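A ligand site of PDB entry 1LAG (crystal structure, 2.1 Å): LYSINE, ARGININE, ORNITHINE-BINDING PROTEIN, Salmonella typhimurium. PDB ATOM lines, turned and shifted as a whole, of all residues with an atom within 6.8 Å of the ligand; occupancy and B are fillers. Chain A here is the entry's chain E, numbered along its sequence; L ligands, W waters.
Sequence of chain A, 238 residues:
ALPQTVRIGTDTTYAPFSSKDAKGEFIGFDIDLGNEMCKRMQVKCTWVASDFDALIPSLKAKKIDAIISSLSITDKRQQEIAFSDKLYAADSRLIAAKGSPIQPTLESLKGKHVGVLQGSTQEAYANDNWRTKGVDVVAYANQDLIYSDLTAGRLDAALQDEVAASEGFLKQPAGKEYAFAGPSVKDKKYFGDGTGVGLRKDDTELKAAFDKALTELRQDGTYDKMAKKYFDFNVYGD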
ATOM      1  N   ASP A  11      12.038  14.436 -35.821  1.00  0.00           N
ATOM      2  CA  ASP A  11      13.382  14.909 -35.914  1.00  0.00           C
ATOM      3  C   ASP A  11      13.909  14.059 -37.059  1.00  0.00           C
ATOM      4  O   ASP A  11      14.186  12.848 -36.989  1.00  0.00           O
ATOM      5  CB  ASP A  11      14.095  14.662 -34.571  1.00  0.00           C
ATOM      6  CG  ASP A  11      15.584  14.347 -34.692  1.00  0.00           C
ATOM      7  OD1 ASP A  11      16.309  15.059 -35.394  1.00  0.00           O
ATOM      8  OD2 ASP A  11      15.993  13.337 -34.128  1.00  0.00           O
ATOM      9  N   THR A  13      16.637  13.503 -38.414  1.00  0.00           N
ATOM     10  CA  THR A  13      18.005  13.043 -38.560  1.00  0.00           C
ATOM     11  C   THR A  13      18.111  11.609 -38.072  1.00  0.00           C
ATOM     12  O   THR A  13      19.107  11.232 -37.445  1.00  0.00           O
ATOM     13  CB  THR A  13      18.925  14.042 -37.785  1.00  0.00           C
ATOM     14  OG1 THR A  13      18.598  14.052 -36.403  1.00  0.00           O
ATOM     15  CG2 THR A  13      18.736  15.462 -38.313  1.00  0.00           C
ATOM     16  N   TYR A  14      17.145  10.734 -38.347  1.00  0.00           N
ATOM     17  CA  TYR A  14      17.240   9.399 -37.789  1.00  0.00           C
ATOM     18  C   TYR A  14      16.805   8.360 -38.802  1.00  0.00           C
ATOM     19  O   TYR A  14      15.794   7.657 -38.655  1.00  0.00           O
ATOM     20  CB  TYR A  14      16.351   9.350 -36.541  1.00  0.00           C
ATOM     21  CG  TYR A  14      16.835   8.475 -35.381  1.00  0.00           C
ATOM     22  CD1 TYR A  14      18.039   8.788 -34.775  1.00  0.00           C
ATOM     23  CD2 TYR A  14      16.068   7.415 -34.936  1.00  0.00           C
ATOM     24  CE1 TYR A  14      18.497   8.040 -33.719  1.00  0.00           C
ATOM     25  CE2 TYR A  14      16.526   6.665 -33.858  1.00  0.00           C
ATOM     26  CZ  TYR A  14      17.734   6.987 -33.269  1.00  0.00           C
ATOM     27  OH  TYR A  14      18.183   6.294 -32.153  1.00  0.00           O
ATOM     28  N   ASP A  30       8.751   6.077 -40.191  1.00  0.00           N
ATOM     29  CA  ASP A  30       7.852   6.864 -39.327  1.00  0.00           C
ATOM     30  C   ASP A  30       6.847   7.739 -40.061  1.00  0.00           C
ATOM     31  O   ASP A  30       5.708   7.929 -39.622  1.00  0.00           O
ATOM     32  CB  ASP A  30       8.589   7.814 -38.406  1.00  0.00           C
ATOM     33  CG  ASP A  30       9.178   7.168 -37.183  1.00  0.00           C
ATOM     34  OD1 ASP A  30       8.853   6.031 -36.867  1.00  0.00           O
ATOM     35  OD2 ASP A  30       9.955   7.826 -36.527  1.00  0.00           O
ATOM     36  N   PHE A  52      15.146  16.750 -31.583  1.00  0.00           N
ATOM     37  CA  PHE A  52      14.546  15.770 -30.719  1.00  0.00           C
ATOM     38  C   PHE A  52      14.258  16.294 -29.342  1.00  0.00           C
ATOM     39  O   PHE A  52      13.133  16.058 -28.896  1.00  0.00           O
ATOM     40  CB  PHE A  52      15.462  14.560 -30.616  1.00  0.00           C
ATOM     41  CG  PHE A  52      14.787  13.404 -29.942  1.00  0.00           C
ATOM     42  CD1 PHE A  52      13.796  12.712 -30.615  1.00  0.00           C
ATOM     43  CD2 PHE A  52      15.119  13.044 -28.654  1.00  0.00           C
ATOM     44  CE1 PHE A  52      13.149  11.660 -30.007  1.00  0.00           C
ATOM     45  CE2 PHE A  52      14.457  11.984 -28.042  1.00  0.00           C
ATOM     46  CZ  PHE A  52      13.481  11.276 -28.719  1.00  0.00           C
ATOM     47  N   LEU A  55      10.883  18.182 -28.878  1.00  0.00           N
ATOM     48  CA  LEU A  55       9.603  17.642 -29.308  1.00  0.00           C
ATOM     49  C   LEU A  55       8.568  17.531 -28.199  1.00  0.00           C
ATOM     50  O   LEU A  55       7.434  17.997 -28.368  1.00  0.00           O
ATOM     51  CB  LEU A  55       9.842  16.249 -29.986  1.00  0.00           C
ATOM     52  CG  LEU A  55      10.525  16.175 -31.375  1.00  0.00           C
ATOM     53  CD1 LEU A  55      10.852  14.729 -31.769  1.00  0.00           C
ATOM     54  CD2 LEU A  55       9.595  16.738 -32.409  1.00  0.00           C
ATOM     55  N   SER A  69       8.663  10.082 -33.950  1.00  0.00           N
ATOM     56  CA  SER A  69      10.092  10.239 -34.020  1.00  0.00           C
ATOM     57  C   SER A  69      10.863   9.144 -33.253  1.00  0.00           C
ATOM     58  O   SER A  69      11.788   9.461 -32.477  1.00  0.00           O
ATOM     59  CB  SER A  69      10.376  11.634 -33.490  1.00  0.00           C
ATOM     60  OG  SER A  69      11.599  12.150 -34.009  1.00  0.00           O
ATOM     61  N   SER A  70      10.505   7.848 -33.465  1.00  0.00           N
ATOM     62  CA  SER A  70      11.075   6.699 -32.732  1.00  0.00           C
ATOM     63  C   SER A  70      11.076   6.999 -31.219  1.00  0.00           C
ATOM     64  O   SER A  70      12.043   6.758 -30.486  1.00  0.00           O
ATOM     65  CB  SER A  70      12.509   6.429 -33.249  1.00  0.00           C
ATOM     66  OG  SER A  70      12.572   5.991 -34.607  1.00  0.00           O
ATOM     67  N   LEU A  71       9.961   7.505 -30.740  1.00  0.00           N
ATOM     68  CA  LEU A  71       9.814   7.905 -29.343  1.00  0.00           C
ATOM     69  C   LEU A  71       9.518   6.704 -28.441  1.00  0.00           C
ATOM     70  O   LEU A  71       8.392   6.196 -28.446  1.00  0.00           O
ATOM     71  CB  LEU A  71       8.693   8.946 -29.252  1.00  0.00           C
ATOM     72  CG  LEU A  71       8.637   9.708 -27.934  1.00  0.00           C
ATOM     73  CD1 LEU A  71       9.854  10.611 -27.820  1.00  0.00           C
ATOM     74  CD2 LEU A  71       7.380  10.546 -27.866  1.00  0.00           C
ATOM     75  N   SER A  72      10.499   6.236 -27.657  1.00  0.00           N
ATOM     76  CA  SER A  72      10.297   5.065 -26.830  1.00  0.00           C
ATOM     77  C   SER A  72       9.267   5.321 -25.729  1.00  0.00           C
ATOM     78  O   SER A  72       9.252   6.405 -25.137  1.00  0.00           O
ATOM     79  CB  SER A  72      11.624   4.641 -26.219  1.00  0.00           C
ATOM     80  OG  SER A  72      12.479   4.200 -27.265  1.00  0.00           O
ATOM     81  N   ILE A  73       8.360   4.372 -25.484  1.00  0.00           N
ATOM     82  CA  ILE A  73       7.352   4.434 -24.430  1.00  0.00           C
ATOM     83  C   ILE A  73       8.071   4.029 -23.141  1.00  0.00           C
ATOM     84  O   ILE A  73       8.525   2.896 -22.997  1.00  0.00           O
ATOM     85  CB  ILE A  73       6.177   3.439 -24.729  1.00  0.00           C
ATOM     86  CG1 ILE A  73       5.645   3.691 -26.149  1.00  0.00           C
ATOM     87  CG2 ILE A  73       5.079   3.616 -23.675  1.00  0.00           C
ATOM     88  CD1 ILE A  73       4.922   2.524 -26.853  1.00  0.00           C
ATOM     89  N   THR A  74       8.283   4.984 -22.220  1.00  0.00           N
ATOM     90  CA  THR A  74       9.018   4.730 -21.001  1.00  0.00           C
ATOM     91  C   THR A  74       8.100   5.251 -19.920  1.00  0.00           C
ATOM     92  O   THR A  74       7.270   6.164 -20.092  1.00  0.00           O
ATOM     93  CB  THR A  74      10.361   5.523 -20.921  1.00  0.00           C
ATOM     94  OG1 THR A  74      10.022   6.919 -20.902  1.00  0.00           O
ATOM     95  CG2 THR A  74      11.297   5.250 -22.090  1.00  0.00           C
ATOM     96  N   ARG A  77       8.444   9.116 -19.480  1.00  0.00           N
ATOM     97  CA  ARG A  77       7.686   9.964 -20.403  1.00  0.00           C
ATOM     98  C   ARG A  77       6.185   9.830 -20.179  1.00  0.00           C
ATOM     99  O   ARG A  77       5.436  10.799 -20.336  1.00  0.00           O
ATOM    100  CB  ARG A  77       8.041   9.583 -21.816  1.00  0.00           C
ATOM    101  CG  ARG A  77       9.440   9.995 -22.111  1.00  0.00           C
ATOM    102  CD  ARG A  77       9.859   9.542 -23.474  1.00  0.00           C
ATOM    103  NE  ARG A  77      11.172  10.074 -23.800  1.00  0.00           N
ATOM    104  CZ  ARG A  77      11.975   9.506 -24.705  1.00  0.00           C
ATOM    105  NH1 ARG A  77      11.613   8.411 -25.357  1.00  0.00           N
ATOM    106  NH2 ARG A  77      13.148  10.047 -25.006  1.00  0.00           N
ATOM    107  N   ALA A  90      12.464  -1.041 -30.206  1.00  0.00           N
ATOM    108  CA  ALA A  90      13.719  -0.384 -30.369  1.00  0.00           C
ATOM    109  C   ALA A  90      14.710  -0.738 -29.271  1.00  0.00           C
ATOM    110  O   ALA A  90      14.570  -0.246 -28.147  1.00  0.00           O
ATOM    111  CB  ALA A  90      13.579   1.157 -30.339  1.00  0.00           C
ATOM    112  N   SER A  92      18.788  -0.606 -27.842  1.00  0.00           N
ATOM    113  CA  SER A  92      19.952   0.241 -27.943  1.00  0.00           C
ATOM    114  C   SER A  92      21.220  -0.581 -28.104  1.00  0.00           C
ATOM    115  O   SER A  92      21.317  -1.670 -27.537  1.00  0.00           O
ATOM    116  CB  SER A  92      20.092   1.110 -26.693  1.00  0.00           C
ATOM    117  OG  SER A  92      19.146   2.146 -26.638  1.00  0.00           O
ATOM    118  N   LEU A 117      22.387  11.160 -28.218  1.00  0.00           N
ATOM    119  CA  LEU A 117      21.489  12.220 -28.599  1.00  0.00           C
ATOM    120  C   LEU A 117      20.926  12.904 -27.341  1.00  0.00           C
ATOM    121  O   LEU A 117      20.390  12.259 -26.416  1.00  0.00           O
ATOM    122  CB  LEU A 117      20.334  11.663 -29.431  1.00  0.00           C
ATOM    123  CG  LEU A 117      19.306  12.647 -29.920  1.00  0.00           C
ATOM    124  CD1 LEU A 117      19.968  13.638 -30.843  1.00  0.00           C
ATOM    125  CD2 LEU A 117      18.210  11.938 -30.652  1.00  0.00           C
ATOM    126  N   GLY A 119      18.440  14.361 -25.084  1.00  0.00           N
ATOM    127  CA  GLY A 119      17.056  14.148 -24.835  1.00  0.00           C
ATOM    128  C   GLY A 119      16.650  12.703 -24.996  1.00  0.00           C
ATOM    129  O   GLY A 119      15.475  12.415 -24.775  1.00  0.00           O
ATOM    130  N   SER A 120      17.485  11.763 -25.389  1.00  0.00           N
ATOM    131  CA  SER A 120      16.978  10.429 -25.637  1.00  0.00           C
ATOM    132  C   SER A 120      17.053   9.579 -24.389  1.00  0.00           C
ATOM    133  O   SER A 120      17.671   9.938 -23.385  1.00  0.00           O
ATOM    134  CB  SER A 120      17.803   9.799 -26.740  1.00  0.00           C
ATOM    135  OG  SER A 120      19.178   9.842 -26.387  1.00  0.00           O
ATOM    136  N   THR A 121      16.540   8.364 -24.439  1.00  0.00           N
ATOM    137  CA  THR A 121      16.695   7.464 -23.310  1.00  0.00           C
ATOM    138  C   THR A 121      18.163   7.079 -23.104  1.00  0.00           C
ATOM    139  O   THR A 121      18.591   6.697 -22.008  1.00  0.00           O
ATOM    140  CB  THR A 121      15.800   6.244 -23.568  1.00  0.00           C
ATOM    141  OG1 THR A 121      16.287   5.686 -24.771  1.00  0.00           O
ATOM    142  CG2 THR A 121      14.326   6.579 -23.629  1.00  0.00           C
ATOM    143  N   GLN A 122      18.954   7.118 -24.187  1.00  0.00           N
ATOM    144  CA  GLN A 122      20.363   6.783 -24.179  1.00  0.00           C
ATOM    145  C   GLN A 122      21.142   7.855 -23.462  1.00  0.00           C
ATOM    146  O   GLN A 122      22.110   7.518 -22.799  1.00  0.00           O
ATOM    147  CB  GLN A 122      20.951   6.669 -25.578  1.00  0.00           C
ATOM    148  CG  GLN A 122      20.520   5.505 -26.434  1.00  0.00           C
ATOM    149  CD  GLN A 122      19.197   5.668 -27.153  1.00  0.00           C
ATOM    150  OE1 GLN A 122      18.709   6.765 -27.417  1.00  0.00           O
ATOM    151  NE2 GLN A 122      18.577   4.578 -27.571  1.00  0.00           N
ATOM    152  N   GLN A 143      21.482  13.305 -34.378  1.00  0.00           N
ATOM    153  CA  GLN A 143      22.263  12.092 -34.578  1.00  0.00           C
ATOM    154  C   GLN A 143      23.210  12.203 -35.745  1.00  0.00           C
ATOM    155  O   GLN A 143      24.171  11.462 -35.820  1.00  0.00           O
ATOM    156  CB  GLN A 143      21.257  10.948 -34.758  1.00  0.00           C
ATOM    157  CG  GLN A 143      21.770   9.518 -34.864  1.00  0.00           C
ATOM    158  CD  GLN A 143      22.388   8.988 -33.586  1.00  0.00           C
ATOM    159  OE1 GLN A 143      23.386   8.283 -33.643  1.00  0.00           O
ATOM    160  NE2 GLN A 143      21.886   9.273 -32.399  1.00  0.00           N
ATOM    161  N   GLN A 160      22.749   4.512 -29.457  1.00  0.00           N
ATOM    162  CA  GLN A 160      21.528   4.949 -30.102  1.00  0.00           C
ATOM    163  C   GLN A 160      20.737   3.667 -30.352  1.00  0.00           C
ATOM    164  O   GLN A 160      21.156   2.572 -29.944  1.00  0.00           O
ATOM    165  CB  GLN A 160      21.779   5.662 -31.460  1.00  0.00           C
ATOM    166  CG  GLN A 160      22.604   4.937 -32.553  1.00  0.00           C
ATOM    167  CD  GLN A 160      24.099   4.809 -32.232  1.00  0.00           C
ATOM    168  OE1 GLN A 160      24.802   5.792 -32.145  1.00  0.00           O
ATOM    169  NE2 GLN A 160      24.661   3.636 -31.918  1.00  0.00           N
ATOM    170  N   ASP A 161      19.608   3.798 -31.036  1.00  0.00           N
ATOM    171  CA  ASP A 161      18.785   2.657 -31.350  1.00  0.00           C
ATOM    172  C   ASP A 161      19.472   1.827 -32.419  1.00  0.00           C
ATOM    173  O   ASP A 161      19.988   2.327 -33.422  1.00  0.00           O
ATOM    174  CB  ASP A 161      17.410   3.130 -31.844  1.00  0.00           C
ATOM    175  CG  ASP A 161      16.492   3.768 -30.808  1.00  0.00           C
ATOM    176  OD1 ASP A 161      16.730   3.699 -29.616  1.00  0.00           O
ATOM    177  OD2 ASP A 161      15.486   4.353 -31.217  1.00  0.00           O
ATOM    178  N   PHE A 191      15.072   2.144 -21.268  1.00  0.00           N
ATOM    179  CA  PHE A 191      14.732   2.169 -22.659  1.00  0.00           C
ATOM    180  C   PHE A 191      13.280   1.931 -23.028  1.00  0.00           C
ATOM    181  O   PHE A 191      12.916   2.038 -24.212  1.00  0.00           O
ATOM    182  CB  PHE A 191      15.671   1.194 -23.331  1.00  0.00           C
ATOM    183  CG  PHE A 191      17.142   1.584 -23.076  1.00  0.00           C
ATOM    184  CD1 PHE A 191      17.610   2.815 -23.444  1.00  0.00           C
ATOM    185  CD2 PHE A 191      18.021   0.662 -22.503  1.00  0.00           C
ATOM    186  CE1 PHE A 191      18.954   3.139 -23.257  1.00  0.00           C
ATOM    187  CE2 PHE A 191      19.358   0.998 -22.311  1.00  0.00           C
ATOM    188  CZ  PHE A 191      19.832   2.239 -22.696  1.00  0.00           C
ATOM    189  N   GLY A 194       9.337  -0.397 -26.839  1.00  0.00           N
ATOM    190  CA  GLY A 194       8.932  -0.054 -28.190  1.00  0.00           C
ATOM    191  C   GLY A 194       8.693   1.452 -28.296  1.00  0.00           C
ATOM    192  O   GLY A 194       8.893   2.196 -27.312  1.00  0.00           O
ATOM    193  N   THR A 195       8.313   1.930 -29.480  1.00  0.00           N
ATOM    194  CA  THR A 195       8.091   3.347 -29.718  1.00  0.00           C
ATOM    195  C   THR A 195       6.605   3.546 -29.955  1.00  0.00           C
ATOM    196  O   THR A 195       5.897   2.584 -30.275  1.00  0.00           O
ATOM    197  CB  THR A 195       8.936   3.805 -30.944  1.00  0.00           C
ATOM    198  OG1 THR A 195       8.430   3.173 -32.114  1.00  0.00           O
ATOM    199  CG2 THR A 195      10.404   3.462 -30.785  1.00  0.00           C
HETATM  200  N1  LIG L   1      14.231   5.715 -28.888  1.00  0.00           N
HETATM  201  C1  LIG L   1      15.147   6.577 -28.253  1.00  0.00           C
HETATM  202  C2  LIG L   1      14.240   7.620 -27.572  1.00  0.00           C
HETATM  203  O1  LIG L   1      13.010   7.593 -27.729  1.00  0.00           O
HETATM  204  C3  LIG L   1      16.105   7.224 -29.260  1.00  0.00           C
HETATM  205  C4  LIG L   1      15.665   8.199 -30.369  1.00  0.00           C
HETATM  206  N2  LIG L   1      16.465   9.030 -31.013  1.00  0.00           N
HETATM  207  C5  LIG L   1      14.438   8.391 -30.898  1.00  0.00           C
HETATM  208  C6  LIG L   1      15.785   9.692 -31.896  1.00  0.00           C
HETATM  209  N3  LIG L   1      14.561   9.312 -31.815  1.00  0.00           N
HETATM  210  O2  LIG L   1      14.794   8.442 -26.881  1.00  0.00           O
HETATM  211  O   HOH W   1      13.911  10.697 -34.581  1.00  0.00           O
HETATM  212  O   HOH W   2      19.379   8.052 -30.170  1.00  0.00           O
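O of Ser 72 sits at hydrogen-bond distance from NH1 of Arg 77. The side-chain hydroxyl of Ser 69 lies within hydrogen-bond range of the backbone NH of Asp 11 (2.9 Å). O of Gly 119 is in hydrogen-bond range of NH2 of Arg 77 (3.3 Å). N of Ser 70 lies within hydrogen-bond range of OD2 of Asp 30 (3.1 Å). The side-chain amide nitrogen of Gln 122 is in hydrogen-bond range of the side-chain carboxylate of Asp 161, 2.9 Å away. OG of Ser 120 sits close to OE1 of Gln 122 (3.3 Å). The backbone carbonyl oxygen (O) of Leu 117 lies within hydrogen-bond range of the side-chain hydroxyl (OG) of Ser 120 (2.7 Å). OG of Ser 92 sits at hydrogen-bond distance from NE2 of Gln 122.
Water W1 lies within hydrogen-bond range of the side-chain hydroxyl of Ser 69 (2.8 Å), a nitrogen (N3) of the ligand (3.2 Å) and the backbone carbonyl oxygen of Asp 11 (3.2 Å). Water W2 lies within hydrogen-bond range of the side-chain hydroxyl of Tyr 14 (2.9 Å), the side-chain amide oxygen of Gln 122 (3.1 Å) and a nitrogen (N2) of the ligand (3.2 Å).
Phe 52 touches the ligand. CA of Leu 71 touches O1 of the ligand (3.6 Å). CD2 of Leu 117 touches N2 of the ligand, 3.4 Å away. Ser 120 touches the ligand (CA to O2, 3.2 Å). Gln 122 touches the ligand. Hydrophobic or aromatic side chains that line the ligand: Tyr 14, Phe 52 and Leu 117. 12 residues have an atom within 4 Å of the ligand: Tyr 14, Phe 52, Ser 69, Ser 70, Leu 71, Ser 72, Arg 77, Leu 117, Ser 120, Thr 121, Gln 122 and Asp 161.
The backbone NH of Ser 72 lies within hydrogen-bond range of an oxygen (O1) of the ligand. OG of Ser 72 is in hydrogen-bond range of N1 of the ligand, at 2.8 Å. O of Ser 69 lies within hydrogen-bond range of N3 of the ligand (2.9 Å). An oxygen (O1) of the ligand lies within salt-bridge range of the guanidinium group of Arg 77 (2.9 Å). The backbone carbonyl oxygen (O) of Ser 70 lies within hydrogen-bond range of a nitrogen (N1) of the ligand (2.9 Å). The side-chain carboxylate (OD2) of Asp 161 lies within salt-bridge range of a nitrogen (N1) of the ligand, at 3.0 Å. The backbone NH (N) of Thr 121 lies within hydrogen-bond range of an oxygen (O2) of the ligand (3.0 Å). N2 of the ligand sits close to OH of Tyr 14 (3.4 Å).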
